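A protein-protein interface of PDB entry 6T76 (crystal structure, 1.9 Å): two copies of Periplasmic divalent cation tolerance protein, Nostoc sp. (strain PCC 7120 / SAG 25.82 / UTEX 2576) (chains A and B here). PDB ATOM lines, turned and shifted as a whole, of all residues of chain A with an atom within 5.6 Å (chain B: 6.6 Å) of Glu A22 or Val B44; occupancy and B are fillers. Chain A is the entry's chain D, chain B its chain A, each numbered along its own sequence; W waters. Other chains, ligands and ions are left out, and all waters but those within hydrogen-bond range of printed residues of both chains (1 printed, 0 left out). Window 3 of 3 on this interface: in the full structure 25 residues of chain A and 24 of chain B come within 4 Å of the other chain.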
ATOM      1  N   ALA A  17      -5.036 -24.968  24.443  1.00  0.00           N
ATOM      2  CA  ALA A  17      -6.204 -24.131  24.716  1.00  0.00           C
ATOM      3  C   ALA A  17      -7.447 -24.668  23.967  1.00  0.00           C
ATOM      4  O   ALA A  17      -8.550 -24.803  24.560  1.00  0.00           O
ATOM      5  CB  ALA A  17      -5.908 -22.643  24.405  1.00  0.00           C
ATOM      6  N   ARG A  18      -7.335 -24.881  22.639  1.00  0.00           N
ATOM      7  CA  ARG A  18      -8.452 -25.328  21.831  1.00  0.00           C
ATOM      8  C   ARG A  18      -9.004 -26.660  22.364  1.00  0.00           C
ATOM      9  O   ARG A  18     -10.207 -26.841  22.438  1.00  0.00           O
ATOM     10  CB  ARG A  18      -8.071 -25.406  20.359  1.00  0.00           C
ATOM     11  CG  ARG A  18      -9.176 -25.987  19.445  1.00  0.00           C
ATOM     12  CD  ARG A  18      -8.748 -26.022  17.963  1.00  0.00           C
ATOM     13  NE  ARG A  18      -7.434 -26.692  17.751  1.00  0.00           N
ATOM     14  CZ  ARG A  18      -7.231 -28.003  17.634  1.00  0.00           C
ATOM     15  NH1 ARG A  18      -8.236 -28.870  17.727  1.00  0.00           N
ATOM     16  NH2 ARG A  18      -6.012 -28.466  17.394  1.00  0.00           N
ATOM     17  N   LEU A  19      -8.108 -27.593  22.701  1.00  0.00           N
ATOM     18  CA  LEU A  19      -8.519 -28.863  23.195  1.00  0.00           C
ATOM     19  C   LEU A  19      -9.265 -28.792  24.550  1.00  0.00           C
ATOM     20  O   LEU A  19     -10.280 -29.486  24.706  1.00  0.00           O
ATOM     21  CB  LEU A  19      -7.335 -29.793  23.383  1.00  0.00           C
ATOM     22  CG  LEU A  19      -6.592 -30.245  22.136  1.00  0.00           C
ATOM     23  CD1 LEU A  19      -5.443 -31.159  22.562  1.00  0.00           C
ATOM     24  CD2 LEU A  19      -7.522 -30.926  21.140  1.00  0.00           C
ATOM     25  N   LEU A  20      -8.809 -27.914  25.442  1.00  0.00           N
ATOM     26  CA  LEU A  20      -9.492 -27.764  26.734  1.00  0.00           C
ATOM     27  C   LEU A  20     -10.921 -27.265  26.541  1.00  0.00           C
ATOM     28  O   LEU A  20     -11.861 -27.688  27.229  1.00  0.00           O
ATOM     29  CB  LEU A  20      -8.728 -26.826  27.637  1.00  0.00           C
ATOM     30  CG  LEU A  20      -7.373 -27.359  28.028  1.00  0.00           C
ATOM     31  CD1 LEU A  20      -6.644 -26.230  28.681  1.00  0.00           C
ATOM     32  CD2 LEU A  20      -7.494 -28.585  28.936  1.00  0.00           C
ATOM     33  N   VAL A  21     -11.109 -26.364  25.602  1.00  0.00           N
ATOM     34  CA  VAL A  21     -12.437 -25.856  25.291  1.00  0.00           C
ATOM     35  C   VAL A  21     -13.300 -26.892  24.558  1.00  0.00           C
ATOM     36  O   VAL A  21     -14.477 -27.030  24.902  1.00  0.00           O
ATOM     37  CB  VAL A  21     -12.369 -24.504  24.551  1.00  0.00           C
ATOM     38  CG1 VAL A  21     -13.749 -23.982  24.153  1.00  0.00           C
ATOM     39  CG2 VAL A  21     -11.649 -23.453  25.371  1.00  0.00           C
ATOM     40  N   GLU A  22     -12.755 -27.582  23.540  1.00  0.00           N
ATOM     41  CA  GLU A  22     -13.483 -28.562  22.822  1.00  0.00           C
ATOM     42  C   GLU A  22     -13.958 -29.695  23.742  1.00  0.00           C
ATOM     43  O   GLU A  22     -15.033 -30.213  23.526  1.00  0.00           O
ATOM     44  CB  GLU A  22     -12.649 -29.164  21.693  1.00  0.00           C
ATOM     45  CG  GLU A  22     -12.446 -28.211  20.518  1.00  0.00           C
ATOM     46  CD  GLU A  22     -11.466 -28.766  19.459  1.00  0.00           C
ATOM     47  OE1 GLU A  22     -10.833 -29.784  19.721  1.00  0.00           O
ATOM     48  OE2 GLU A  22     -11.328 -28.191  18.357  1.00  0.00           O
ATOM     49  N   GLU A  23     -13.146 -30.055  24.738  1.00  0.00           N
ATOM     50  CA  GLU A  23     -13.518 -31.090  25.655  1.00  0.00           C
ATOM     51  C   GLU A  23     -14.332 -30.567  26.854  1.00  0.00           C
ATOM     52  O   GLU A  23     -14.679 -31.340  27.703  1.00  0.00           O
ATOM     53  CB  GLU A  23     -12.274 -31.770  26.159  1.00  0.00           C
ATOM     54  CG  GLU A  23     -11.505 -32.545  25.094  1.00  0.00           C
ATOM     55  CD  GLU A  23     -10.081 -32.896  25.506  1.00  0.00           C
ATOM     56  OE1 GLU A  23      -9.745 -32.735  26.708  1.00  0.00           O
ATOM     57  OE2 GLU A  23      -9.273 -33.254  24.616  1.00  0.00           O
ATOM     58  N   HIS A  24     -14.616 -29.265  26.912  1.00  0.00           N
ATOM     59  CA  HIS A  24     -15.436 -28.669  27.959  1.00  0.00           C
ATOM     60  C   HIS A  24     -14.826 -28.827  29.318  1.00  0.00           C
ATOM     61  O   HIS A  24     -15.530 -28.964  30.330  1.00  0.00           O
ATOM     62  CB  HIS A  24     -16.876 -29.211  27.934  1.00  0.00           C
ATOM     63  CG  HIS A  24     -17.572 -28.908  26.653  1.00  0.00           C
ATOM     64  ND1 HIS A  24     -18.034 -27.643  26.354  1.00  0.00           N
ATOM     65  CD2 HIS A  24     -17.796 -29.666  25.555  1.00  0.00           C
ATOM     66  CE1 HIS A  24     -18.519 -27.636  25.126  1.00  0.00           C
ATOM     67  NE2 HIS A  24     -18.387 -28.852  24.621  1.00  0.00           N
ATOM     68  N   ILE B  37     -10.448 -18.047  23.187  1.00  0.00           N
ATOM     69  CA  ILE B  37     -11.056 -19.218  22.648  1.00  0.00           C
ATOM     70  C   ILE B  37     -12.113 -19.625  23.703  1.00  0.00           C
ATOM     71  O   ILE B  37     -11.790 -19.739  24.882  1.00  0.00           O
ATOM     72  CB  ILE B  37     -10.040 -20.343  22.484  1.00  0.00           C
ATOM     73  CG1 ILE B  37      -8.915 -19.912  21.533  1.00  0.00           C
ATOM     74  CG2 ILE B  37     -10.741 -21.543  21.900  1.00  0.00           C
ATOM     75  CD1 ILE B  37      -7.812 -20.931  21.432  1.00  0.00           C
ATOM     76  N   TYR B  38     -13.354 -19.795  23.301  1.00  0.00           N
ATOM     77  CA  TYR B  38     -14.376 -20.116  24.296  1.00  0.00           C
ATOM     78  C   TYR B  38     -15.535 -20.883  23.695  1.00  0.00           C
ATOM     79  O   TYR B  38     -15.705 -20.945  22.482  1.00  0.00           O
ATOM     80  CB  TYR B  38     -14.862 -18.880  25.040  1.00  0.00           C
ATOM     81  CG  TYR B  38     -15.453 -17.825  24.174  1.00  0.00           C
ATOM     82  CD1 TYR B  38     -14.645 -16.866  23.568  1.00  0.00           C
ATOM     83  CD2 TYR B  38     -16.805 -17.803  23.900  1.00  0.00           C
ATOM     84  CE1 TYR B  38     -15.187 -15.907  22.728  1.00  0.00           C
ATOM     85  CE2 TYR B  38     -17.355 -16.832  23.094  1.00  0.00           C
ATOM     86  CZ  TYR B  38     -16.543 -15.898  22.502  1.00  0.00           C
ATOM     87  OH  TYR B  38     -17.111 -14.960  21.688  1.00  0.00           O
ATOM     88  N   SER B  39     -16.260 -21.504  24.606  1.00  0.00           N
ATOM     89  CA  SER B  39     -17.396 -22.318  24.323  1.00  0.00           C
ATOM     90  C   SER B  39     -18.626 -21.400  24.363  1.00  0.00           C
ATOM     91  O   SER B  39     -18.820 -20.647  25.319  1.00  0.00           O
ATOM     92  CB  SER B  39     -17.485 -23.410  25.413  1.00  0.00           C
ATOM     93  OG  SER B  39     -18.160 -24.500  24.902  1.00  0.00           O
ATOM     94  N   TRP B  40     -19.453 -21.484  23.326  1.00  0.00           N
ATOM     95  CA  TRP B  40     -20.662 -20.694  23.263  1.00  0.00           C
ATOM     96  C   TRP B  40     -21.734 -21.412  22.431  1.00  0.00           C
ATOM     97  O   TRP B  40     -21.600 -21.577  21.221  1.00  0.00           O
ATOM     98  CB  TRP B  40     -20.382 -19.301  22.690  1.00  0.00           C
ATOM     99  CG  TRP B  40     -21.573 -18.393  22.784  1.00  0.00           C
ATOM    100  CD1 TRP B  40     -22.431 -18.083  21.780  1.00  0.00           C
ATOM    101  CD2 TRP B  40     -22.071 -17.731  23.962  1.00  0.00           C
ATOM    102  NE1 TRP B  40     -23.433 -17.266  22.258  1.00  0.00           N
ATOM    103  CE2 TRP B  40     -23.236 -17.034  23.593  1.00  0.00           C
ATOM    104  CE3 TRP B  40     -21.657 -17.675  25.287  1.00  0.00           C
ATOM    105  CZ2 TRP B  40     -23.989 -16.265  24.513  1.00  0.00           C
ATOM    106  CZ3 TRP B  40     -22.404 -16.917  26.203  1.00  0.00           C
ATOM    107  CH2 TRP B  40     -23.554 -16.219  25.809  1.00  0.00           C
ATOM    108  N   GLY B  42     -22.837 -24.439  21.949  1.00  0.00           N
ATOM    109  CA  GLY B  42     -22.437 -25.589  21.145  1.00  0.00           C
ATOM    110  C   GLY B  42     -21.295 -25.336  20.173  1.00  0.00           C
ATOM    111  O   GLY B  42     -20.957 -26.205  19.384  1.00  0.00           O
ATOM    112  N   GLU B  43     -20.703 -24.150  20.201  1.00  0.00           N
ATOM    113  CA  GLU B  43     -19.615 -23.836  19.272  1.00  0.00           C
ATOM    114  C   GLU B  43     -18.373 -23.361  19.996  1.00  0.00           C
ATOM    115  O   GLU B  43     -18.470 -22.826  21.093  1.00  0.00           O
ATOM    116  CB  GLU B  43     -20.078 -22.794  18.264  1.00  0.00           C
ATOM    117  CG  GLU B  43     -21.042 -23.400  17.263  1.00  0.00           C
ATOM    118  CD  GLU B  43     -21.065 -22.615  15.988  1.00  0.00           C
ATOM    119  OE1 GLU B  43     -21.472 -23.176  14.956  1.00  0.00           O
ATOM    120  OE2 GLU B  43     -20.650 -21.436  16.036  1.00  0.00           O
ATOM    121  N   VAL B  44     -17.224 -23.604  19.378  1.00  0.00           N
ATOM    122  CA  VAL B  44     -15.955 -23.078  19.838  1.00  0.00           C
ATOM    123  C   VAL B  44     -15.677 -21.779  19.077  1.00  0.00           C
ATOM    124  O   VAL B  44     -15.570 -21.767  17.869  1.00  0.00           O
ATOM    125  CB  VAL B  44     -14.813 -24.066  19.588  1.00  0.00           C
ATOM    126  CG1 VAL B  44     -13.495 -23.448  20.011  1.00  0.00           C
ATOM    127  CG2 VAL B  44     -15.086 -25.380  20.308  1.00  0.00           C
ATOM    128  N   CYS B  45     -15.604 -20.689  19.798  1.00  0.00           N
ATOM    129  CA  CYS B  45     -15.384 -19.379  19.214  1.00  0.00           C
ATOM    130  C   CYS B  45     -13.934 -18.942  19.420  1.00  0.00           C
ATOM    131  O   CYS B  45     -13.364 -19.170  20.492  1.00  0.00           O
ATOM    132  CB  CYS B  45     -16.303 -18.363  19.889  1.00  0.00           C
ATOM    133  SG  CYS B  45     -18.024 -18.745  19.567  1.00  0.00           S
ATOM    134  N   SER B  46     -13.359 -18.284  18.411  1.00  0.00           N
ATOM    135  CA  SER B  46     -11.992 -17.833  18.464  1.00  0.00           C
ATOM    136  C   SER B  46     -11.969 -16.356  18.071  1.00  0.00           C
ATOM    137  O   SER B  46     -12.358 -16.030  16.957  1.00  0.00           O
ATOM    138  CB  SER B  46     -11.199 -18.683  17.474  1.00  0.00           C
ATOM    139  OG  SER B  46      -9.856 -18.259  17.434  1.00  0.00           O
HETATM  140  O   HOH W   1     -15.995 -25.457  27.084  1.00  0.00           O
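Hydrophobic or aromatic side chains of chain B that line the printed part of chain A: Ile B37 and Val B44.
Of the 8 printed residues of chain A, 4 touch a printed residue of chain B.
Printed residues of chain A that touch a printed residue of chain B: Ala A17, Val A21, Glu A22 and His A24.
The backbone carbonyl oxygen of Tyr B38 sits at hydrogen-bond distance from the backbone NH of Cys B45 (2.7 Å).
The guanidinium group (NH1) of Arg A18 is in salt-bridge range of the side-chain carboxylate (OE2) of Glu A22, 3.2 Å away.
Water W1 lies within hydrogen-bond range of ND1 of His A24 (3.1 Å), O of Val A21 (3.1 Å) and OG of Ser B39 (3.2 Å).
No position is printed for both chains.
Of the 6 pairs that touch across the chains among the printed residues, none has its exchanged pair printed and touching as well.
Among the printed residues, merely in contact across the chains: Ala A17 with Ile B37 (3.9 Å), Val A21 with Ile B37 (3.7 Å), Val A21 with Tyr B38 (3.6 Å), Val A21 with Ser B39 (3.6 Å) and Glu A22 with Val B44 (3.9 Å).
Of chain B, only Val B44 (3.9 Å) comes within 4 Å of Glu A22.
Of chain A, only Glu A22 comes within 4 Å of Val B44.
Of the printed residues of chain B, Ala A17 touches Ile B37.
Of the printed residues of chain B, Val A21 touches Ile B37 (3.7 Å), Tyr B38 (3.6 Å) and Ser B39 (3.6 Å).
The nearest residue of chain A that does not touch Val B44 is Val A21 (4.2 Å).
The nearest printed residue of chain A that does not touch Ile B37 is Arg A18 (4.2 Å).
OG of Ser B39 sits close to ND1 of His A24, at 3.5 Å.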
